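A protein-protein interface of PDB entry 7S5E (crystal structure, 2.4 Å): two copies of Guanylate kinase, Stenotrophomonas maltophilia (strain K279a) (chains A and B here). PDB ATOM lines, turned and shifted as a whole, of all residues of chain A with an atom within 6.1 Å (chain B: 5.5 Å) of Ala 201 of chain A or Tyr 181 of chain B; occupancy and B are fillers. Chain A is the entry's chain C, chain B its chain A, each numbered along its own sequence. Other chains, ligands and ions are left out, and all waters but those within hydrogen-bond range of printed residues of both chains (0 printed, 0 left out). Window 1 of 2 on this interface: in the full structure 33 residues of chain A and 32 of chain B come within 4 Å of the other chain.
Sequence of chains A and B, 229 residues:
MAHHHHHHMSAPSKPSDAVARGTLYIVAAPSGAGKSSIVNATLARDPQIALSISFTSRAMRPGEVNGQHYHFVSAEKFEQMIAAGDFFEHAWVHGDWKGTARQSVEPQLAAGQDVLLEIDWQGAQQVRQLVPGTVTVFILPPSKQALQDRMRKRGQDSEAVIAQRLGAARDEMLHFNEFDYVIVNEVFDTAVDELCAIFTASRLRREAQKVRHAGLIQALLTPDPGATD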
ATOM      1  N   TYR A 181      19.238   4.410  19.526  1.00  0.00           N
ATOM      2  CA  TYR A 181      18.307   4.868  18.498  1.00  0.00           C
ATOM      3  C   TYR A 181      16.866   4.734  18.974  1.00  0.00           C
ATOM      4  O   TYR A 181      16.546   3.868  19.793  1.00  0.00           O
ATOM      5  CB  TYR A 181      18.476   4.091  17.179  1.00  0.00           C
ATOM      6  CG  TYR A 181      19.872   4.135  16.600  1.00  0.00           C
ATOM      7  CD1 TYR A 181      20.855   3.251  17.024  1.00  0.00           C
ATOM      8  CD2 TYR A 181      20.213   5.082  15.646  1.00  0.00           C
ATOM      9  CE1 TYR A 181      22.123   3.295  16.494  1.00  0.00           C
ATOM     10  CE2 TYR A 181      21.475   5.133  15.119  1.00  0.00           C
ATOM     11  CZ  TYR A 181      22.427   4.243  15.543  1.00  0.00           C
ATOM     12  OH  TYR A 181      23.692   4.318  15.010  1.00  0.00           O
ATOM     13  N   CYS A 196      16.135  -1.412   9.406  1.00  0.00           N
ATOM     14  CA  CYS A 196      17.113  -1.921   8.447  1.00  0.00           C
ATOM     15  C   CYS A 196      18.240  -0.920   8.237  1.00  0.00           C
ATOM     16  O   CYS A 196      19.418  -1.300   8.177  1.00  0.00           O
ATOM     17  CB  CYS A 196      16.425  -2.244   7.119  1.00  0.00           C
ATOM     18  SG  CYS A 196      15.316  -3.671   7.168  1.00  0.00           S
ATOM     19  N   ALA A 197      17.903   0.368   8.171  1.00  0.00           N
ATOM     20  CA  ALA A 197      18.923   1.394   8.004  1.00  0.00           C
ATOM     21  C   ALA A 197      19.902   1.375   9.168  1.00  0.00           C
ATOM     22  O   ALA A 197      21.112   1.565   8.979  1.00  0.00           O
ATOM     23  CB  ALA A 197      18.270   2.770   7.867  1.00  0.00           C
ATOM     24  N   ILE A 198      19.392   1.141  10.381  1.00  0.00           N
ATOM     25  CA  ILE A 198      20.253   1.087  11.555  1.00  0.00           C
ATOM     26  C   ILE A 198      21.198  -0.101  11.466  1.00  0.00           C
ATOM     27  O   ILE A 198      22.397   0.021  11.753  1.00  0.00           O
ATOM     28  CB  ILE A 198      19.395   1.044  12.831  1.00  0.00           C
ATOM     29  CG1 ILE A 198      18.642   2.361  13.001  1.00  0.00           C
ATOM     30  CG2 ILE A 198      20.237   0.729  14.055  1.00  0.00           C
ATOM     31  CD1 ILE A 198      17.622   2.324  14.107  1.00  0.00           C
ATOM     32  N   PHE A 199      20.689  -1.260  11.047  1.00  0.00           N
ATOM     33  CA  PHE A 199      21.555  -2.424  10.903  1.00  0.00           C
ATOM     34  C   PHE A 199      22.621  -2.176   9.845  1.00  0.00           C
ATOM     35  O   PHE A 199      23.805  -2.452  10.067  1.00  0.00           O
ATOM     36  CB  PHE A 199      20.737  -3.671  10.552  1.00  0.00           C
ATOM     37  CG  PHE A 199      19.989  -4.276  11.715  1.00  0.00           C
ATOM     38  CD1 PHE A 199      18.750  -3.811  12.088  1.00  0.00           C
ATOM     39  CD2 PHE A 199      20.516  -5.346  12.411  1.00  0.00           C
ATOM     40  CE1 PHE A 199      18.062  -4.382  13.146  1.00  0.00           C
ATOM     41  CE2 PHE A 199      19.816  -5.919  13.468  1.00  0.00           C
ATOM     42  CZ  PHE A 199      18.592  -5.427  13.830  1.00  0.00           C
ATOM     43  N   THR A 200      22.219  -1.631   8.694  1.00  0.00           N
ATOM     44  CA  THR A 200      23.186  -1.365   7.633  1.00  0.00           C
ATOM     45  C   THR A 200      24.252  -0.388   8.109  1.00  0.00           C
ATOM     46  O   THR A 200      25.457  -0.655   7.984  1.00  0.00           O
ATOM     47  CB  THR A 200      22.471  -0.829   6.392  1.00  0.00           C
ATOM     48  OG1 THR A 200      21.586  -1.830   5.890  1.00  0.00           O
ATOM     49  CG2 THR A 200      23.473  -0.527   5.304  1.00  0.00           C
ATOM     50  N   ALA A 201      23.826   0.718   8.727  1.00  0.00           N
ATOM     51  CA  ALA A 201      24.777   1.728   9.178  1.00  0.00           C
ATOM     52  C   ALA A 201      25.759   1.156  10.195  1.00  0.00           C
ATOM     53  O   ALA A 201      26.951   1.473  10.163  1.00  0.00           O
ATOM     54  CB  ALA A 201      24.032   2.920   9.775  1.00  0.00           C
ATOM     55  N   SER A 202      25.282   0.295  11.094  1.00  0.00           N
ATOM     56  CA  SER A 202      26.165  -0.218  12.130  1.00  0.00           C
ATOM     57  C   SER A 202      27.315  -1.020  11.538  1.00  0.00           C
ATOM     58  O   SER A 202      28.432  -0.973  12.062  1.00  0.00           O
ATOM     59  CB  SER A 202      25.366  -1.066  13.118  1.00  0.00           C
ATOM     60  OG  SER A 202      24.377  -0.280  13.754  1.00  0.00           O
ATOM     61  N   ARG A 203      27.079  -1.729  10.433  1.00  0.00           N
ATOM     62  CA  ARG A 203      28.153  -2.505   9.822  1.00  0.00           C
ATOM     63  C   ARG A 203      29.178  -1.632   9.113  1.00  0.00           C
ATOM     64  O   ARG A 203      30.288  -2.101   8.838  1.00  0.00           O
ATOM     65  CB  ARG A 203      27.577  -3.527   8.844  1.00  0.00           C
ATOM     66  CG  ARG A 203      26.631  -4.504   9.488  1.00  0.00           C
ATOM     67  CD  ARG A 203      26.225  -5.579   8.520  1.00  0.00           C
ATOM     68  NE  ARG A 203      25.163  -6.404   9.078  1.00  0.00           N
ATOM     69  CZ  ARG A 203      23.880  -6.289   8.770  1.00  0.00           C
ATOM     70  NH1 ARG A 203      23.462  -5.425   7.862  1.00  0.00           N
ATOM     71  NH2 ARG A 203      22.993  -7.074   9.378  1.00  0.00           N
ATOM     72  N   LEU A 204      28.839  -0.383   8.819  1.00  0.00           N
ATOM     73  CA  LEU A 204      29.751   0.519   8.141  1.00  0.00           C
ATOM     74  C   LEU A 204      30.616   1.297   9.120  1.00  0.00           C
ATOM     75  O   LEU A 204      31.415   2.140   8.694  1.00  0.00           O
ATOM     76  CB  LEU A 204      28.952   1.494   7.261  1.00  0.00           C
ATOM     77  CG  LEU A 204      28.028   0.817   6.239  1.00  0.00           C
ATOM     78  CD1 LEU A 204      27.089   1.810   5.583  1.00  0.00           C
ATOM     79  CD2 LEU A 204      28.812   0.038   5.194  1.00  0.00           C
ATOM     80  N   ARG A 205      30.447   1.067  10.420  1.00  0.00           N
ATOM     81  CA  ARG A 205      31.235   1.802  11.395  1.00  0.00           C
ATOM     82  C   ARG A 205      32.713   1.482  11.228  1.00  0.00           C
ATOM     83  O   ARG A 205      33.095   0.374  10.837  1.00  0.00           O
ATOM     84  CB  ARG A 205      30.770   1.493  12.823  1.00  0.00           C
ATOM     85  CG  ARG A 205      29.408   2.109  13.173  1.00  0.00           C
ATOM     86  CD  ARG A 205      28.965   1.757  14.585  1.00  0.00           C
ATOM     87  NE  ARG A 205      28.788   0.323  14.739  1.00  0.00           N
ATOM     88  CZ  ARG A 205      28.422  -0.267  15.865  1.00  0.00           C
ATOM     89  NH1 ARG A 205      28.166   0.434  16.957  1.00  0.00           N
ATOM     90  NH2 ARG A 205      28.329  -1.594  15.901  1.00  0.00           N
ATOM     91  N   ARG A 206      33.539   2.480  11.545  1.00  0.00           N
ATOM     92  CA  ARG A 206      34.963   2.420  11.260  1.00  0.00           C
ATOM     93  C   ARG A 206      35.599   1.146  11.797  1.00  0.00           C
ATOM     94  O   ARG A 206      36.278   0.418  11.065  1.00  0.00           O
ATOM     95  CB  ARG A 206      35.645   3.650  11.858  1.00  0.00           C
ATOM     96  CG  ARG A 206      37.162   3.613  11.741  1.00  0.00           C
ATOM     97  CD  ARG A 206      37.804   4.708  12.576  1.00  0.00           C
ATOM     98  NE  ARG A 206      37.560   4.616  14.015  1.00  0.00           N
ATOM     99  CZ  ARG A 206      36.691   5.370  14.678  1.00  0.00           C
ATOM    100  NH1 ARG A 206      35.948   6.272  14.061  1.00  0.00           N
ATOM    101  NH2 ARG A 206      36.594   5.241  15.999  1.00  0.00           N
ATOM    102  N   GLN A 209      34.726  -1.942   9.885  1.00  0.00           N
ATOM    103  CA  GLN A 209      35.246  -1.960   8.520  1.00  0.00           C
ATOM    104  C   GLN A 209      36.758  -2.152   8.482  1.00  0.00           C
ATOM    105  O   GLN A 209      37.280  -2.761   7.541  1.00  0.00           O
ATOM    106  CB  GLN A 209      34.856  -0.674   7.800  1.00  0.00           C
ATOM    107  CG  GLN A 209      33.380  -0.584   7.447  1.00  0.00           C
ATOM    108  CD  GLN A 209      33.003  -1.485   6.293  1.00  0.00           C
ATOM    109  OE1 GLN A 209      33.100  -2.706   6.383  1.00  0.00           O
ATOM    110  NE2 GLN A 209      32.583  -0.883   5.191  1.00  0.00           N
ATOM    111  N   VAL B 135      28.610  14.119  11.596  1.00  0.00           N
ATOM    112  CA  VAL B 135      28.625  12.735  11.135  1.00  0.00           C
ATOM    113  C   VAL B 135      29.564  12.683   9.939  1.00  0.00           C
ATOM    114  O   VAL B 135      29.308  13.325   8.913  1.00  0.00           O
ATOM    115  CB  VAL B 135      27.212  12.255  10.765  1.00  0.00           C
ATOM    116  CG1 VAL B 135      27.224  10.809  10.279  1.00  0.00           C
ATOM    117  CG2 VAL B 135      26.285  12.409  11.951  1.00  0.00           C
ATOM    118  N   THR B 136      30.659  11.926  10.067  1.00  0.00           N
ATOM    119  CA  THR B 136      31.708  11.894   9.052  1.00  0.00           C
ATOM    120  C   THR B 136      31.845  10.502   8.441  1.00  0.00           C
ATOM    121  O   THR B 136      31.790   9.492   9.151  1.00  0.00           O
ATOM    122  CB  THR B 136      33.061  12.365   9.630  1.00  0.00           C
ATOM    123  OG1 THR B 136      33.504  11.472  10.655  1.00  0.00           O
ATOM    124  CG2 THR B 136      32.921  13.761  10.215  1.00  0.00           C
ATOM    125  N   VAL B 137      31.968  10.463   7.110  1.00  0.00           N
ATOM    126  CA  VAL B 137      32.057   9.228   6.337  1.00  0.00           C
ATOM    127  C   VAL B 137      33.257   9.307   5.399  1.00  0.00           C
ATOM    128  O   VAL B 137      33.506  10.348   4.785  1.00  0.00           O
ATOM    129  CB  VAL B 137      30.765   8.967   5.538  1.00  0.00           C
ATOM    130  CG1 VAL B 137      30.893   7.678   4.744  1.00  0.00           C
ATOM    131  CG2 VAL B 137      29.550   8.920   6.471  1.00  0.00           C
ATOM    132  N   PHE B 138      34.014   8.219   5.301  1.00  0.00           N
ATOM    133  CA  PHE B 138      35.137   8.113   4.377  1.00  0.00           C
ATOM    134  C   PHE B 138      34.837   7.043   3.335  1.00  0.00           C
ATOM    135  O   PHE B 138      34.354   5.956   3.675  1.00  0.00           O
ATOM    136  CB  PHE B 138      36.439   7.776   5.112  1.00  0.00           C
ATOM    137  CG  PHE B 138      37.684   8.146   4.345  1.00  0.00           C
ATOM    138  CD1 PHE B 138      38.149   9.452   4.340  1.00  0.00           C
ATOM    139  CD2 PHE B 138      38.375   7.198   3.622  1.00  0.00           C
ATOM    140  CE1 PHE B 138      39.285   9.794   3.641  1.00  0.00           C
ATOM    141  CE2 PHE B 138      39.510   7.539   2.924  1.00  0.00           C
ATOM    142  CZ  PHE B 138      39.965   8.840   2.935  1.00  0.00           C
ATOM    143  N   PHE B 179      37.299   9.088  10.689  1.00  0.00           N
ATOM    144  CA  PHE B 179      35.918   9.171  10.245  1.00  0.00           C
ATOM    145  C   PHE B 179      35.067   8.096  10.923  1.00  0.00           C
ATOM    146  O   PHE B 179      35.551   7.004  11.233  1.00  0.00           O
ATOM    147  CB  PHE B 179      35.874   9.055   8.713  1.00  0.00           C
ATOM    148  CG  PHE B 179      36.494  10.239   8.027  1.00  0.00           C
ATOM    149  CD1 PHE B 179      37.878  10.366   7.948  1.00  0.00           C
ATOM    150  CD2 PHE B 179      35.709  11.247   7.508  1.00  0.00           C
ATOM    151  CE1 PHE B 179      38.463  11.470   7.354  1.00  0.00           C
ATOM    152  CE2 PHE B 179      36.289  12.361   6.914  1.00  0.00           C
ATOM    153  CZ  PHE B 179      37.670  12.470   6.835  1.00  0.00           C
ATOM    154  N   ASP B 180      33.783   8.414  11.142  1.00  0.00           N
ATOM    155  CA  ASP B 180      32.911   7.504  11.884  1.00  0.00           C
ATOM    156  C   ASP B 180      32.584   6.263  11.069  1.00  0.00           C
ATOM    157  O   ASP B 180      32.538   5.153  11.613  1.00  0.00           O
ATOM    158  CB  ASP B 180      31.617   8.202  12.310  1.00  0.00           C
ATOM    159  CG  ASP B 180      31.854   9.420  13.186  1.00  0.00           C
ATOM    160  OD1 ASP B 180      32.583   9.305  14.194  1.00  0.00           O
ATOM    161  OD2 ASP B 180      31.269  10.485  12.894  1.00  0.00           O
ATOM    162  N   TYR B 181      32.362   6.432   9.765  1.00  0.00           N
ATOM    163  CA  TYR B 181      31.941   5.362   8.875  1.00  0.00           C
ATOM    164  C   TYR B 181      32.915   5.249   7.714  1.00  0.00           C
ATOM    165  O   TYR B 181      33.587   6.217   7.340  1.00  0.00           O
ATOM    166  CB  TYR B 181      30.523   5.601   8.332  1.00  0.00           C
ATOM    167  CG  TYR B 181      29.499   5.745   9.433  1.00  0.00           C
ATOM    168  CD1 TYR B 181      29.319   6.962  10.072  1.00  0.00           C
ATOM    169  CD2 TYR B 181      28.713   4.663   9.835  1.00  0.00           C
ATOM    170  CE1 TYR B 181      28.401   7.105  11.077  1.00  0.00           C
ATOM    171  CE2 TYR B 181      27.782   4.798  10.849  1.00  0.00           C
ATOM    172  CZ  TYR B 181      27.635   6.029  11.465  1.00  0.00           C
ATOM    173  OH  TYR B 181      26.730   6.223  12.478  1.00  0.00           O
ATOM    174  N   VAL B 182      33.010   4.048   7.164  1.00  0.00           N
ATOM    175  CA  VAL B 182      33.833   3.790   5.994  1.00  0.00           C
ATOM    176  C   VAL B 182      32.982   3.053   4.982  1.00  0.00           C
ATOM    177  O   VAL B 182      32.317   2.068   5.323  1.00  0.00           O
ATOM    178  CB  VAL B 182      35.099   2.988   6.344  1.00  0.00           C
ATOM    179  CG1 VAL B 182      35.860   2.645   5.092  1.00  0.00           C
ATOM    180  CG2 VAL B 182      35.979   3.796   7.300  1.00  0.00           C
ATOM    181  N   ILE B 183      32.992   3.530   3.743  1.00  0.00           N
ATOM    182  CA  ILE B 183      32.305   2.870   2.644  1.00  0.00           C
ATOM    183  C   ILE B 183      33.346   2.448   1.620  1.00  0.00           C
ATOM    184  O   ILE B 183      34.195   3.253   1.221  1.00  0.00           O
ATOM    185  CB  ILE B 183      31.233   3.777   2.012  1.00  0.00           C
ATOM    186  CG1 ILE B 183      30.135   4.087   3.032  1.00  0.00           C
ATOM    187  CG2 ILE B 183      30.666   3.162   0.743  1.00  0.00           C
ATOM    188  CD1 ILE B 183      29.039   4.991   2.495  1.00  0.00           C
ATOM    189  N   ALA B 197      21.735   4.821   4.142  1.00  0.00           N
ATOM    190  CA  ALA B 197      21.501   4.195   5.436  1.00  0.00           C
ATOM    191  C   ALA B 197      22.111   5.019   6.563  1.00  0.00           C
ATOM    192  O   ALA B 197      21.467   5.243   7.595  1.00  0.00           O
ATOM    193  CB  ALA B 197      22.066   2.775   5.434  1.00  0.00           C
ATOM    194  N   ILE B 198      23.326   5.539   6.354  1.00  0.00           N
ATOM    195  CA  ILE B 198      23.986   6.326   7.391  1.00  0.00           C
ATOM    196  C   ILE B 198      23.210   7.610   7.662  1.00  0.00           C
ATOM    197  O   ILE B 198      23.033   8.022   8.815  1.00  0.00           O
ATOM    198  CB  ILE B 198      25.440   6.631   6.982  1.00  0.00           C
ATOM    199  CG1 ILE B 198      26.262   5.349   6.882  1.00  0.00           C
ATOM    200  CG2 ILE B 198      26.097   7.603   7.968  1.00  0.00           C
ATOM    201  CD1 ILE B 198      27.647   5.586   6.292  1.00  0.00           C
ATOM    202  N   ALA B 201      19.977   6.644   9.498  1.00  0.00           N
ATOM    203  CA  ALA B 201      20.251   6.229  10.872  1.00  0.00           C
ATOM    204  C   ALA B 201      20.566   7.418  11.766  1.00  0.00           C
ATOM    205  O   ALA B 201      20.182   7.437  12.939  1.00  0.00           O
ATOM    206  CB  ALA B 201      21.399   5.218  10.905  1.00  0.00           C
ATOM    207  N   ARG B 205      18.984   8.703  15.832  1.00  0.00           N
ATOM    208  CA  ARG B 205      19.756   8.722  17.061  1.00  0.00           C
ATOM    209  C   ARG B 205      18.923   9.321  18.183  1.00  0.00           C
ATOM    210  O   ARG B 205      18.040  10.148  17.952  1.00  0.00           O
ATOM    211  CB  ARG B 205      21.037   9.520  16.864  1.00  0.00           C
ATOM    212  CG  ARG B 205      22.065   8.800  16.034  1.00  0.00           C
ATOM    213  CD  ARG B 205      23.270   9.685  15.826  1.00  0.00           C
ATOM    214  NE  ARG B 205      24.226   9.083  14.905  1.00  0.00           N
ATOM    215  CZ  ARG B 205      25.432   9.573  14.644  1.00  0.00           C
ATOM    216  NH1 ARG B 205      25.860  10.695  15.209  1.00  0.00           N
ATOM    217  NH2 ARG B 205      26.231   8.916  13.805  1.00  0.00           N
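The backbone carbonyl oxygen of Asp 180 of chain B is in hydrogen-bond range of the backbone NH of Arg 206 of chain A, at 2.9 Å. The side-chain amide nitrogen (NE2) of Gln 209 of chain A lies within hydrogen-bond range of the backbone carbonyl oxygen (O) of Val 182 of chain B (3.0 Å). The backbone carbonyl oxygen (O) of Leu 204 of chain A sits at hydrogen-bond distance from the backbone NH (N) of Val 182 of chain B (2.9 Å). NH1 of Arg 206 of chain A sits at hydrogen-bond distance from O of Phe 179 of chain B, at 2.9 Å.
The side-chain hydroxyl (OH) of Tyr 181 of chain B sits at hydrogen-bond distance from the guanidinium group (NH2) of Arg 205 of chain B, 3.0 Å away. O of Tyr 181 of chain B is in hydrogen-bond range of N of Phe 138 of chain B, 2.9 Å away. The backbone carbonyl oxygen (O) of Thr 136 of chain B sits at hydrogen-bond distance from the backbone NH (N) of Asp 180 of chain B. The backbone carbonyl oxygen (O) of Thr 136 of chain B lies within hydrogen-bond range of the backbone NH (N) of Tyr 181 of chain B. The backbone carbonyl oxygen (O) of Cys 196 of chain A is in hydrogen-bond range of the side-chain hydroxyl (OG1) of Thr 200 of chain A. The guanidinium group (NE) of Arg 205 of chain A sits at hydrogen-bond distance from the backbone carbonyl oxygen (O) of Ser 202 of chain A (3.0 Å).
CE2 of Tyr 181 of chain A touches O of Ala 201 of chain B, 3.4 Å away. CE2 of Tyr 181 of chain A touches CG of Arg 205 of chain B (3.8 Å). Ala 197 of chain B touches Ala 197 of chain A (CB to O, 3.9 Å). Ala 197 of chain B touches Thr 200 of chain A (CB to CG2, 3.6 Å). Ala 201 of chain A touches Tyr 181 of chain B (O to CE2, 3.5 Å). CB of Ala 201 of chain A touches CB of Ala 201 of chain B, 3.7 Å away. Leu 204 of chain A touches Tyr 181 of chain B (O to CA, 3.3 Å). CG1 of Ile 198 of chain B touches CD1 of Leu 204 of chain A, at 3.9 Å. Asp 180 of chain B touches Arg 205 of chain A. CE2 of Tyr 181 of chain B touches CG of Arg 205 of chain A, at 3.9 Å.
Ala 201 of chain A touches two residues of chain B. Of the printed residues of chain B, Arg 206 of chain A touches Phe 179 and Asp 180. Thr 136 of chain B touches none of the printed residues of chain A. Phe 138 of chain B touches none of the printed residues of chain A. Tyr 181 of chain B touches three residues of chain A. Printed residues of chain A within 4 Å of Ile 198 of chain B: Leu 204.
Of the 13 printed residues of chain A, 8 touch a printed residue of chain B. Printed residues of chain A that touch a printed residue of chain B: Tyr 181, Ala 197, Thr 200, Ala 201, Leu 204, Arg 205, Arg 206 and Gln 209. Of the 13 printed residues of chain B, 8 touch a printed residue of chain A. Hydrophobic or aromatic side chains of chain B within 4 Å of the printed part of chain A: Tyr 181, Val 182, Ala 197, Ile 198 and Ala 201. Along chain B the printed residues that touch a printed residue of chain A span positions 179 to 205. Among the printed residues, 14 pairs touch across the chains. Among the printed residues, no Asp or Glu carboxylate lies within 4 Å of a Lys or Arg side-chain nitrogen of the other chain.
Tyr 181 of chain A touches Ala 201 of chain B, and with the chains exchanged Ala 201 of chain A touches Tyr 181 of chain B. Tyr 181 of chain A touches Arg 205 of chain B, and with the chains exchanged Arg 205 of chain A touches Tyr 181 of chain B. Ala 197 of chain B touches its own counterpart, Ala 197 of chain A. Ala 201 of chain B touches its own counterpart, Ala 201 of chain A. Positions printed for both chains: 181, 197, 198, 201 and 205. Of the 14 pairs that touch across the chains among the printed residues, 6 have their exchanged pair printed and touching as well.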
